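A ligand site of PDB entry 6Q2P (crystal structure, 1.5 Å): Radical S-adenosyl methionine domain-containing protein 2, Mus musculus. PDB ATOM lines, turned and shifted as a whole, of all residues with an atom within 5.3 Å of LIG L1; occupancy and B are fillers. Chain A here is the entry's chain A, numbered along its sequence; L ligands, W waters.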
ATOM      1  N   HIS A  35     -10.434 -34.295   7.737  1.00  0.00           N
ATOM      2  CA  HIS A  35     -11.667 -34.362   8.531  1.00  0.00           C
ATOM      3  C   HIS A  35     -11.347 -35.182   9.783  1.00  0.00           C
ATOM      4  O   HIS A  35     -11.586 -36.385   9.860  1.00  0.00           O
ATOM      5  CB  HIS A  35     -12.778 -35.011   7.723  1.00  0.00           C
ATOM      6  CG  HIS A  35     -13.151 -34.267   6.474  1.00  0.00           C
ATOM      7  ND1 HIS A  35     -14.416 -33.778   6.255  1.00  0.00           N
ATOM      8  CD2 HIS A  35     -12.426 -33.946   5.368  1.00  0.00           C
ATOM      9  CE1 HIS A  35     -14.458 -33.178   5.075  1.00  0.00           C
ATOM     10  NE2 HIS A  35     -13.267 -33.267   4.510  1.00  0.00           N
ATOM     11  N   CYS A  40     -20.571 -33.934  15.135  1.00  0.00           N
ATOM     12  CA  CYS A  40     -21.097 -32.602  14.859  1.00  0.00           C
ATOM     13  C   CYS A  40     -22.194 -32.254  15.855  1.00  0.00           C
ATOM     14  O   CYS A  40     -22.830 -33.126  16.454  1.00  0.00           O
ATOM     15  CB  CYS A  40     -21.653 -32.465  13.442  1.00  0.00           C
ATOM     16  SG  CYS A  40     -21.873 -30.724  13.009  1.00  0.00           S
ATOM     17  N   PHE A  46     -28.701 -32.565   4.503  1.00  0.00           N
ATOM     18  CA  PHE A  46     -27.946 -33.062   3.359  1.00  0.00           C
ATOM     19  C   PHE A  46     -26.521 -33.470   3.703  1.00  0.00           C
ATOM     20  O   PHE A  46     -25.764 -33.820   2.805  1.00  0.00           O
ATOM     21  CB  PHE A  46     -27.891 -31.992   2.243  1.00  0.00           C
ATOM     22  CG  PHE A  46     -27.440 -30.633   2.726  1.00  0.00           C
ATOM     23  CD1 PHE A  46     -26.142 -30.431   3.186  1.00  0.00           C
ATOM     24  CD2 PHE A  46     -28.317 -29.561   2.735  1.00  0.00           C
ATOM     25  CE1 PHE A  46     -25.736 -29.180   3.649  1.00  0.00           C
ATOM     26  CE2 PHE A  46     -27.911 -28.310   3.199  1.00  0.00           C
ATOM     27  CZ  PHE A  46     -26.617 -28.120   3.638  1.00  0.00           C
ATOM     28  N   CYS A  47     -26.122 -33.409   4.977  1.00  0.00           N
ATOM     29  CA  CYS A  47     -24.714 -33.564   5.356  1.00  0.00           C
ATOM     30  C   CYS A  47     -24.080 -34.761   4.670  1.00  0.00           C
ATOM     31  O   CYS A  47     -24.570 -35.889   4.777  1.00  0.00           O
ATOM     32  CB  CYS A  47     -24.625 -33.743   6.863  1.00  0.00           C
ATOM     33  SG  CYS A  47     -22.893 -33.904   7.416  1.00  0.00           S
ATOM     34  N   PHE A  48     -22.961 -34.521   3.978  1.00  0.00           N
ATOM     35  CA  PHE A  48     -22.239 -35.588   3.294  1.00  0.00           C
ATOM     36  C   PHE A  48     -21.016 -36.095   4.054  1.00  0.00           C
ATOM     37  O   PHE A  48     -20.233 -36.869   3.504  1.00  0.00           O
ATOM     38  CB  PHE A  48     -21.927 -35.261   1.808  1.00  0.00           C
ATOM     39  CG  PHE A  48     -20.928 -34.119   1.575  1.00  0.00           C
ATOM     40  CD1 PHE A  48     -20.232 -33.502   2.610  1.00  0.00           C
ATOM     41  CD2 PHE A  48     -20.699 -33.692   0.280  1.00  0.00           C
ATOM     42  CE1 PHE A  48     -19.327 -32.454   2.336  1.00  0.00           C
ATOM     43  CE2 PHE A  48     -19.800 -32.667   0.002  1.00  0.00           C
ATOM     44  CZ  PHE A  48     -19.126 -32.044   1.037  1.00  0.00           C
ATOM     45  N   HIS A  49     -20.850 -35.703   5.325  1.00  0.00           N
ATOM     46  CA  HIS A  49     -19.717 -36.189   6.112  1.00  0.00           C
ATOM     47  C   HIS A  49     -20.204 -36.402   7.540  1.00  0.00           C
ATOM     48  O   HIS A  49     -19.976 -35.566   8.428  1.00  0.00           O
ATOM     49  CB  HIS A  49     -18.486 -35.294   6.034  1.00  0.00           C
ATOM     50  CG  HIS A  49     -17.228 -36.028   6.366  1.00  0.00           C
ATOM     51  ND1 HIS A  49     -16.496 -36.714   5.432  1.00  0.00           N
ATOM     52  CD2 HIS A  49     -16.623 -36.267   7.563  1.00  0.00           C
ATOM     53  CE1 HIS A  49     -15.482 -37.322   6.022  1.00  0.00           C
ATOM     54  NE2 HIS A  49     -15.540 -37.072   7.312  1.00  0.00           N
ATOM     55  N   SER A  80     -11.424 -29.966   8.645  1.00  0.00           N
ATOM     56  CA  SER A  80     -12.854 -30.112   8.387  1.00  0.00           C
ATOM     57  C   SER A  80     -13.390 -31.205   9.312  1.00  0.00           C
ATOM     58  O   SER A  80     -12.742 -31.596  10.290  1.00  0.00           O
ATOM     59  CB  SER A  80     -13.057 -30.395   6.893  1.00  0.00           C
ATOM     60  OG  SER A  80     -14.430 -30.314   6.529  1.00  0.00           O
ATOM     61  N   GLY A  81     -14.580 -31.711   8.990  1.00  0.00           N
ATOM     62  CA  GLY A  81     -15.220 -32.737   9.788  1.00  0.00           C
ATOM     63  C   GLY A  81     -16.551 -33.139   9.153  1.00  0.00           C
ATOM     64  O   GLY A  81     -16.634 -33.175   7.926  1.00  0.00           O
ATOM     65  N   GLY A  82     -17.605 -33.398   9.938  1.00  0.00           N
ATOM     66  CA  GLY A  82     -17.657 -33.084  11.358  1.00  0.00           C
ATOM     67  C   GLY A  82     -17.500 -31.591  11.648  1.00  0.00           C
ATOM     68  O   GLY A  82     -17.241 -30.791  10.730  1.00  0.00           O
ATOM     69  N   GLU A  83     -17.629 -31.206  12.911  1.00  0.00           N
ATOM     70  CA  GLU A  83     -17.386 -29.825  13.295  1.00  0.00           C
ATOM     71  C   GLU A  83     -16.037 -29.747  13.969  1.00  0.00           C
ATOM     72  O   GLU A  83     -15.895 -30.233  15.105  1.00  0.00           O
ATOM     73  CB  GLU A  83     -18.486 -29.286  14.201  1.00  0.00           C
ATOM     74  CG  GLU A  83     -18.201 -27.886  14.761  1.00  0.00           C
ATOM     75  CD  GLU A  83     -17.693 -26.918  13.699  1.00  0.00           C
ATOM     76  OE1 GLU A  83     -18.231 -26.936  12.569  1.00  0.00           O
ATOM     77  OE2 GLU A  83     -16.730 -26.167  13.986  1.00  0.00           O
ATOM     78  N   PRO A  84     -15.009 -29.175  13.330  1.00  0.00           N
ATOM     79  CA  PRO A  84     -13.653 -29.283  13.880  1.00  0.00           C
ATOM     80  C   PRO A  84     -13.464 -28.605  15.226  1.00  0.00           C
ATOM     81  O   PRO A  84     -12.571 -29.011  15.984  1.00  0.00           O
ATOM     82  CB  PRO A  84     -12.771 -28.651  12.787  1.00  0.00           C
ATOM     83  CG  PRO A  84     -13.691 -27.858  11.947  1.00  0.00           C
ATOM     84  CD  PRO A  84     -15.036 -28.525  12.004  1.00  0.00           C
ATOM     85  N   VAL A 112     -12.762 -25.109   7.724  1.00  0.00           N
ATOM     86  CA  VAL A 112     -14.181 -24.952   7.394  1.00  0.00           C
ATOM     87  C   VAL A 112     -14.965 -25.344   8.625  1.00  0.00           C
ATOM     88  O   VAL A 112     -14.763 -26.437   9.177  1.00  0.00           O
ATOM     89  CB  VAL A 112     -14.583 -25.799   6.171  1.00  0.00           C
ATOM     90  CG1 VAL A 112     -16.066 -25.614   5.887  1.00  0.00           C
ATOM     91  CG2 VAL A 112     -13.780 -25.410   4.952  1.00  0.00           C
ATOM     92  N   SER A 113     -15.845 -24.451   9.084  1.00  0.00           N
ATOM     93  CA  SER A 113     -16.563 -24.655  10.330  1.00  0.00           C
ATOM     94  C   SER A 113     -17.995 -24.154  10.218  1.00  0.00           C
ATOM     95  O   SER A 113     -18.278 -23.228   9.457  1.00  0.00           O
ATOM     96  CB  SER A 113     -15.840 -23.888  11.445  1.00  0.00           C
ATOM     97  OG  SER A 113     -16.584 -23.863  12.648  1.00  0.00           O
ATOM     98  N   ASN A 114     -18.891 -24.748  11.018  1.00  0.00           N
ATOM     99  CA  ASN A 114     -20.244 -24.201  11.130  1.00  0.00           C
ATOM    100  C   ASN A 114     -20.309 -22.922  11.949  1.00  0.00           C
ATOM    101  O   ASN A 114     -21.356 -22.264  11.971  1.00  0.00           O
ATOM    102  CB  ASN A 114     -21.281 -25.255  11.588  1.00  0.00           C
ATOM    103  CG  ASN A 114     -21.110 -25.713  13.051  1.00  0.00           C
ATOM    104  OD1 ASN A 114     -20.582 -24.981  13.897  1.00  0.00           O
ATOM    105  ND2 ASN A 114     -21.579 -26.915  13.340  1.00  0.00           N
ATOM    106  N   ILE A 135     -16.659 -20.071   7.123  1.00  0.00           N
ATOM    107  CA  ILE A 135     -17.871 -20.388   7.860  1.00  0.00           C
ATOM    108  C   ILE A 135     -18.927 -20.805   6.864  1.00  0.00           C
ATOM    109  O   ILE A 135     -19.149 -20.130   5.856  1.00  0.00           O
ATOM    110  CB  ILE A 135     -18.364 -19.198   8.707  1.00  0.00           C
ATOM    111  CG1 ILE A 135     -17.241 -18.691   9.628  1.00  0.00           C
ATOM    112  CG2 ILE A 135     -19.592 -19.616   9.520  1.00  0.00           C
ATOM    113  CD1 ILE A 135     -16.709 -19.746  10.591  1.00  0.00           C
ATOM    114  N   SER A 136     -19.598 -21.929   7.141  1.00  0.00           N
ATOM    115  CA  SER A 136     -20.681 -22.383   6.286  1.00  0.00           C
ATOM    116  C   SER A 136     -21.947 -21.614   6.597  1.00  0.00           C
ATOM    117  O   SER A 136     -22.361 -21.517   7.759  1.00  0.00           O
ATOM    118  CB  SER A 136     -20.899 -23.895   6.437  1.00  0.00           C
ATOM    119  OG  SER A 136     -19.762 -24.578   5.961  1.00  0.00           O
ATOM    120  N   ASP A 138     -25.659 -21.279   4.578  1.00  0.00           N
ATOM    121  CA  ASP A 138     -26.460 -21.634   3.415  1.00  0.00           C
ATOM    122  C   ASP A 138     -27.598 -20.671   3.170  1.00  0.00           C
ATOM    123  O   ASP A 138     -28.174 -20.678   2.066  1.00  0.00           O
ATOM    124  CB  ASP A 138     -27.028 -23.039   3.602  1.00  0.00           C
ATOM    125  CG  ASP A 138     -25.953 -24.089   3.805  1.00  0.00           C
ATOM    126  OD1 ASP A 138     -24.876 -23.980   3.188  1.00  0.00           O
ATOM    127  OD2 ASP A 138     -26.201 -25.023   4.597  1.00  0.00           O
ATOM    128  N   ARG A 150     -29.404 -26.211  10.244  1.00  0.00           N
ATOM    129  CA  ARG A 150     -28.230 -25.453  10.698  1.00  0.00           C
ATOM    130  C   ARG A 150     -28.538 -24.825  12.041  1.00  0.00           C
ATOM    131  O   ARG A 150     -28.996 -23.680  12.120  1.00  0.00           O
ATOM    132  CB  ARG A 150     -27.906 -24.354   9.700  1.00  0.00           C
ATOM    133  CG  ARG A 150     -27.306 -24.820   8.447  1.00  0.00           C
ATOM    134  CD  ARG A 150     -25.790 -24.935   8.540  1.00  0.00           C
ATOM    135  NE  ARG A 150     -25.292 -25.323   7.240  1.00  0.00           N
ATOM    136  CZ  ARG A 150     -24.104 -25.849   6.974  1.00  0.00           C
ATOM    137  NH1 ARG A 150     -23.204 -26.067   7.933  1.00  0.00           N
ATOM    138  NH2 ARG A 150     -23.819 -26.177   5.722  1.00  0.00           N
ATOM    139  N   ASN A 178     -18.818 -20.533   2.847  1.00  0.00           N
ATOM    140  CA  ASN A 178     -19.228 -21.643   1.993  1.00  0.00           C
ATOM    141  C   ASN A 178     -20.739 -21.770   2.052  1.00  0.00           C
ATOM    142  O   ASN A 178     -21.317 -21.729   3.143  1.00  0.00           O
ATOM    143  CB  ASN A 178     -18.660 -22.966   2.500  1.00  0.00           C
ATOM    144  CG  ASN A 178     -17.174 -23.096   2.263  1.00  0.00           C
ATOM    145  OD1 ASN A 178     -16.518 -22.169   1.777  1.00  0.00           O
ATOM    146  ND2 ASN A 178     -16.621 -24.259   2.609  1.00  0.00           N
ATOM    147  N   VAL A 180     -24.082 -24.239   0.534  1.00  0.00           N
ATOM    148  CA  VAL A 180     -24.598 -25.405  -0.179  1.00  0.00           C
ATOM    149  C   VAL A 180     -25.920 -25.013  -0.799  1.00  0.00           C
ATOM    150  O   VAL A 180     -26.891 -24.709  -0.083  1.00  0.00           O
ATOM    151  CB  VAL A 180     -24.789 -26.599   0.774  1.00  0.00           C
ATOM    152  CG1 VAL A 180     -25.381 -27.792  -0.004  1.00  0.00           C
ATOM    153  CG2 VAL A 180     -23.464 -26.971   1.420  1.00  0.00           C
ATOM    154  N   PHE A 205     -21.482 -24.447  -3.515  1.00  0.00           N
ATOM    155  CA  PHE A 205     -21.504 -25.876  -3.852  1.00  0.00           C
ATOM    156  C   PHE A 205     -22.915 -26.296  -4.244  1.00  0.00           C
ATOM    157  O   PHE A 205     -23.883 -26.001  -3.533  1.00  0.00           O
ATOM    158  CB  PHE A 205     -21.168 -26.719  -2.615  1.00  0.00           C
ATOM    159  CG  PHE A 205     -19.887 -26.358  -1.916  1.00  0.00           C
ATOM    160  CD1 PHE A 205     -18.693 -26.229  -2.613  1.00  0.00           C
ATOM    161  CD2 PHE A 205     -19.883 -26.199  -0.533  1.00  0.00           C
ATOM    162  CE1 PHE A 205     -17.501 -25.931  -1.946  1.00  0.00           C
ATOM    163  CE2 PHE A 205     -18.695 -25.905   0.156  1.00  0.00           C
ATOM    164  CZ  PHE A 205     -17.510 -25.758  -0.554  1.00  0.00           C
ATOM    165  N   GLN A 206     -23.049 -27.039  -5.335  1.00  0.00           N
ATOM    166  CA  GLN A 206     -24.308 -27.741  -5.569  1.00  0.00           C
ATOM    167  C   GLN A 206     -24.424 -28.881  -4.557  1.00  0.00           C
ATOM    168  O   GLN A 206     -23.442 -29.590  -4.295  1.00  0.00           O
ATOM    169  CB  GLN A 206     -24.331 -28.293  -6.990  1.00  0.00           C
ATOM    170  CG  GLN A 206     -25.691 -28.897  -7.378  1.00  0.00           C
ATOM    171  CD  GLN A 206     -25.661 -29.551  -8.751  1.00  0.00           C
ATOM    172  OE1 GLN A 206     -24.618 -29.658  -9.385  1.00  0.00           O
ATOM    173  NE2 GLN A 206     -26.838 -30.000  -9.215  1.00  0.00           N
ATOM    174  N   CYS A 207     -25.600 -29.054  -3.973  1.00  0.00           N
ATOM    175  CA  CYS A 207     -25.783 -30.138  -3.018  1.00  0.00           C
ATOM    176  C   CYS A 207     -25.408 -31.470  -3.672  1.00  0.00           C
ATOM    177  O   CYS A 207     -25.846 -31.767  -4.783  1.00  0.00           O
ATOM    178  CB  CYS A 207     -27.235 -30.177  -2.562  1.00  0.00           C
ATOM    179  SG  CYS A 207     -27.536 -31.252  -1.156  1.00  0.00           S
ATOM    180  N   LEU A 208     -24.568 -32.252  -2.993  1.00  0.00           N
ATOM    181  CA  LEU A 208     -23.950 -33.447  -3.558  1.00  0.00           C
ATOM    182  C   LEU A 208     -24.400 -34.700  -2.803  1.00  0.00           C
ATOM    183  O   LEU A 208     -24.394 -34.726  -1.568  1.00  0.00           O
ATOM    184  CB  LEU A 208     -22.424 -33.321  -3.495  1.00  0.00           C
ATOM    185  CG  LEU A 208     -21.610 -34.506  -4.015  1.00  0.00           C
ATOM    186  CD1 LEU A 208     -21.774 -34.646  -5.529  1.00  0.00           C
ATOM    187  CD2 LEU A 208     -20.133 -34.308  -3.667  1.00  0.00           C
ATOM    188  N   LEU A 209     -24.757 -35.741  -3.555  1.00  0.00           N
ATOM    189  CA  LEU A 209     -25.173 -37.020  -2.994  1.00  0.00           C
ATOM    190  C   LEU A 209     -23.963 -37.938  -2.866  1.00  0.00           C
ATOM    191  O   LEU A 209     -23.194 -38.103  -3.821  1.00  0.00           O
ATOM    192  CB  LEU A 209     -26.206 -37.628  -3.947  1.00  0.00           C
ATOM    193  CG  LEU A 209     -27.271 -38.589  -3.455  1.00  0.00           C
ATOM    194  CD1 LEU A 209     -28.124 -37.950  -2.362  1.00  0.00           C
ATOM    195  CD2 LEU A 209     -28.129 -39.026  -4.645  1.00  0.00           C
ATOM    196  N   ASN A 214     -25.211 -39.588   2.832  1.00  0.00           N
ATOM    197  CA  ASN A 214     -26.537 -38.975   2.737  1.00  0.00           C
ATOM    198  C   ASN A 214     -27.417 -39.672   1.697  1.00  0.00           C
ATOM    199  O   ASN A 214     -28.385 -39.070   1.231  1.00  0.00           O
ATOM    200  CB  ASN A 214     -26.412 -37.476   2.456  1.00  0.00           C
ATOM    201  CG  ASN A 214     -25.740 -37.190   1.138  1.00  0.00           C
ATOM    202  OD1 ASN A 214     -25.555 -38.090   0.324  1.00  0.00           O
ATOM    203  ND2 ASN A 214     -25.357 -35.925   0.927  1.00  0.00           N
ATOM    204  N   ALA A 223     -30.228 -37.036   1.539  1.00  0.00           N
ATOM    205  CA  ALA A 223     -30.153 -35.744   0.880  1.00  0.00           C
ATOM    206  C   ALA A 223     -31.031 -35.629  -0.365  1.00  0.00           C
ATOM    207  O   ALA A 223     -31.085 -34.531  -0.942  1.00  0.00           O
ATOM    208  CB  ALA A 223     -28.704 -35.426   0.480  1.00  0.00           C
ATOM    209  N   MET A 254     -17.060 -30.717  -7.926  1.00  0.00           N
ATOM    210  CA  MET A 254     -16.775 -30.909  -6.511  1.00  0.00           C
ATOM    211  C   MET A 254     -16.412 -32.341  -6.142  1.00  0.00           C
ATOM    212  O   MET A 254     -15.570 -32.537  -5.260  1.00  0.00           O
ATOM    213  CB  MET A 254     -17.998 -30.497  -5.683  1.00  0.00           C
ATOM    214  CG  MET A 254     -17.735 -30.465  -4.191  1.00  0.00           C
ATOM    215  SD  MET A 254     -19.193 -30.021  -3.241  1.00  0.00           S
ATOM    216  CE  MET A 254     -18.431 -29.686  -1.646  1.00  0.00           C
HETATM  217  N1  LIG L   1     -19.125 -28.893   9.909  1.00  0.00           N
HETATM  218  C1  LIG L   1     -18.345 -27.964   9.089  1.00  0.00           C
HETATM  219  C2  LIG L   1     -17.297 -28.677   8.228  1.00  0.00           C
HETATM  220  C3  LIG L   1     -17.739 -30.039   7.659  1.00  0.00           C
HETATM  221  S1  LIG L   1     -18.758 -29.930   6.161  1.00  0.00           S
HETATM  222  C4  LIG L   1     -19.254 -27.125   8.220  1.00  0.00           C
HETATM  223  O1  LIG L   1     -20.419 -27.412   8.000  1.00  0.00           O
HETATM  224  O2  LIG L   1     -18.766 -26.014   7.701  1.00  0.00           O
HETATM  225  C5  LIG L   1     -17.602 -29.183   4.977  1.00  0.00           C
HETATM  226  C6  LIG L   1     -18.326 -28.373   3.884  1.00  0.00           C
HETATM  227  O3  LIG L   1     -19.118 -29.262   3.065  1.00  0.00           O
HETATM  228  C7  LIG L   1     -19.266 -27.308   4.486  1.00  0.00           C
HETATM  229  O4  LIG L   1     -19.107 -26.075   3.800  1.00  0.00           O
HETATM  230  C8  LIG L   1     -20.667 -27.934   4.249  1.00  0.00           C
HETATM  231  O5  LIG L   1     -21.715 -26.966   4.201  1.00  0.00           O
HETATM  232  C9  LIG L   1     -20.418 -28.656   2.896  1.00  0.00           C
HETATM  233  N2  LIG L   1     -21.390 -29.714   2.668  1.00  0.00           N
HETATM  234  C10 LIG L   1     -21.963 -30.557   3.586  1.00  0.00           C
HETATM  235  N3  LIG L   1     -22.779 -31.386   2.987  1.00  0.00           N
HETATM  236  C11 LIG L   1     -22.747 -31.121   1.640  1.00  0.00           C
HETATM  237  C12 LIG L   1     -23.401 -31.655   0.510  1.00  0.00           C
HETATM  238  N4  LIG L   1     -24.287 -32.689   0.638  1.00  0.00           N
HETATM  239  N5  LIG L   1     -23.112 -31.130  -0.687  1.00  0.00           N
HETATM  240  C13 LIG L   1     -22.252 -30.121  -0.823  1.00  0.00           C
HETATM  241  N6  LIG L   1     -21.620 -29.581   0.212  1.00  0.00           N
HETATM  242  C14 LIG L   1     -21.857 -30.060   1.434  1.00  0.00           C
HETATM  243 FE1  LG2 L   2     -22.334 -30.711  10.781  1.00  0.00          FE
HETATM  244 FE2  LG2 L   2     -23.891 -29.481   8.933  1.00  0.00          FE
HETATM  245 FE3  LG2 L   2     -22.568 -31.781   8.362  1.00  0.00          FE
HETATM  246 FE4  LG2 L   2     -21.108 -29.347   8.796  1.00  0.00          FE
HETATM  247  S1  LG2 L   2     -22.632 -29.887   7.070  1.00  0.00           S
HETATM  248  S2  LG2 L   2     -20.703 -31.629   9.521  1.00  0.00           S
HETATM  249  S3  LG2 L   2     -22.565 -28.438  10.403  1.00  0.00           S
HETATM  250  S4  LG2 L   2     -24.240 -31.537   9.937  1.00  0.00           S
HETATM  251  N1  LG3 L   3     -15.659 -32.665   0.509  1.00  0.00           N
HETATM  252  C1  LG3 L   3     -16.225 -33.841   0.851  1.00  0.00           C
HETATM  253  N2  LG3 L   3     -16.568 -34.727  -0.098  1.00  0.00           N
HETATM  254  C2  LG3 L   3     -16.365 -34.459  -1.383  1.00  0.00           C
HETATM  255  C3  LG3 L   3     -15.797 -33.219  -1.768  1.00  0.00           C
HETATM  256  C4  LG3 L   3     -15.447 -32.329  -0.802  1.00  0.00           C
HETATM  257  O1  LG3 L   3     -16.408 -34.100   2.036  1.00  0.00           O
HETATM  258  N3  LG3 L   3     -16.712 -35.390  -2.340  1.00  0.00           N
HETATM  259  C5  LG3 L   3     -15.294 -31.718   1.563  1.00  0.00           C
HETATM  260  C6  LG3 L   3     -13.835 -31.230   1.412  1.00  0.00           C
HETATM  261  O2  LG3 L   3     -12.882 -32.175   1.936  1.00  0.00           O
HETATM  262  C7  LG3 L   3     -13.906 -29.920   2.239  1.00  0.00           C
HETATM  263  C8  LG3 L   3     -15.331 -29.427   1.952  1.00  0.00           C
HETATM  264  O3  LG3 L   3     -16.062 -30.526   1.389  1.00  0.00           O
HETATM  265  O4  LG3 L   3     -13.747 -30.179   3.653  1.00  0.00           O
HETATM  266  C9  LG3 L   3     -15.352 -28.308   0.920  1.00  0.00           C
HETATM  267  O5  LG3 L   3     -14.874 -27.136   1.571  1.00  0.00           O
HETATM  268  P1  LG3 L   3     -13.897 -26.140   0.799  1.00  0.00           P
HETATM  269  O6  LG3 L   3     -14.138 -26.164  -0.659  1.00  0.00           O
HETATM  270  O7  LG3 L   3     -14.006 -24.703   1.451  1.00  0.00           O
HETATM  271  O8  LG3 L   3     -12.440 -26.737   1.092  1.00  0.00           O
HETATM  272  P2  LG3 L   3     -10.982 -26.138   0.883  1.00  0.00           P
HETATM  273  O9  LG3 L   3     -10.062 -27.271   0.607  1.00  0.00           O
HETATM  274  O10 LG3 L   3     -10.568 -25.231   2.111  1.00  0.00           O
HETATM  275  O11 LG3 L   3     -11.172 -25.210  -0.411  1.00  0.00           O
HETATM  276  P3  LG3 L   3     -10.236 -24.139  -1.126  1.00  0.00           P
HETATM  277  O12 LG3 L   3     -10.573 -24.245  -2.665  1.00  0.00           O
HETATM  278  O13 LG3 L   3      -8.749 -24.557  -0.780  1.00  0.00           O
HETATM  279  O14 LG3 L   3     -10.589 -22.826  -0.566  1.00  0.00           O
HETATM  280  O   HOH W   1     -22.183 -24.441   3.451  1.00  0.00           O
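ND2 of Asn 214 lies close to N4 of LIG L1 (3.4 Å). OG of Ser 136 is in hydrogen-bond range of O2 of LIG L1, 2.5 Å away. An iron atom (FE1) of LG2 L2 is bound by the side-chain sulfur (SG) of Cys 40 (2.3 Å). O of Leu 208 is in hydrogen-bond range of N4 of LIG L1, 3.0 Å away. OE1 of Glu 83 lies close to N1 of LIG L1 (3.4 Å). ND2 of Asn 178 is in hydrogen-bond range of O4 of LIG L1 (3.3 Å). N of Gly 82 sits close to S2 of LG2 L2 (3.6 Å). ND2 of Asn 114 lies close to S3 of LG2 L2. O5 of LIG L1 sits at hydrogen-bond distance from NH2 of Arg 150 (2.7 Å). The side-chain amide nitrogen (ND2) of Asn 178 is in hydrogen-bond range of an oxygen (O7) of LG3 L3 (2.9 Å). O4 of LG3 L3 is in hydrogen-bond range of OG of Ser 80 (3.0 Å). O of Phe 46 lies within hydrogen-bond range of N4 of LIG L1 (2.9 Å). NE2 of His 35 lies within hydrogen-bond range of O2 of LG3 L3, 2.8 Å away. An iron atom (FE3) of LG2 L2 is bound by the side-chain sulfur (SG) of Cys 47, 2.3 Å away. A sulfur (S3) of LG2 L2 sits close to the guanidinium group (NH1) of Arg 150 (3.5 Å). N of Phe 48 sits at hydrogen-bond distance from N3 of LIG L1, at 3.3 Å. The backbone carbonyl oxygen (O) of Gly 82 sits close to a nitrogen (N1) of LIG L1 (2.8 Å). N of Leu 208 lies within hydrogen-bond range of N5 of LIG L1.
Water W1 lies within hydrogen-bond range of an oxygen (O5) of LIG L1, the side-chain carboxylate of Asp 138, the backbone carbonyl oxygen of Asn 178, the guanidinium group of Arg 150, the backbone NH of Val 180 and the side-chain hydroxyl of Ser 136.
O of Ser 113 lies close to O2 of LIG L1 (3.3 Å). Merely in contact with LIG L1: Cys 47 (3.8 Å), Ser 80 (3.5 Å), Gly 81 (3.3 Å), Val 112 (3.3 Å), Asn 114 (3.6 Å), Val 180 (3.3 Å), Phe 205 (3.7 Å), Gln 206 (3.7 Å), Cys 207 (3.7 Å) and Met 254 (3.7 Å). Hydrophobic or aromatic side chains that line LIG L1: Phe 46, Phe 48, Val 112, Val 180, Phe 205, Leu 208 and Met 254. 20 residues have an atom within 4 Å of LIG L1: Phe 46, Cys 47, Phe 48, Ser 80, Gly 81, Gly 82, Glu 83, Val 112, Ser 113, Asn 114, Ser 136, Arg 150, Asn 178, Val 180, Phe 205, Gln 206, Cys 207, Leu 208, Asn 214 and Met 254.
O1 of LIG L1 is bound to FE4 of LG2 L2, at 2.2 Å.
The side-chain carboxylate (OE1) of Glu 83 is in hydrogen-bond range of the backbone NH (N) of Asn 114 (2.8 Å). The backbone NH of Asn 178 lies within hydrogen-bond range of the backbone carbonyl oxygen of Ile 135, 3.1 Å away. N of Ala 223 sits at hydrogen-bond distance from O of Asn 214. The side-chain carboxylate of Glu 83 lies within hydrogen-bond range of the side-chain hydroxyl of Ser 113 (2.7 Å). The side-chain carboxylate (OD1) of Asp 138 lies within hydrogen-bond range of the backbone NH (N) of Val 180, at 2.8 Å. SG of Cys 47 sits close to N of His 49, at 3.4 Å. The side-chain amide nitrogen of Asn 214 sits at hydrogen-bond distance from the backbone carbonyl oxygen of Phe 46, at 2.9 Å. The guanidinium group of Arg 150 is in salt-bridge range of the side-chain carboxylate of Asp 138.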
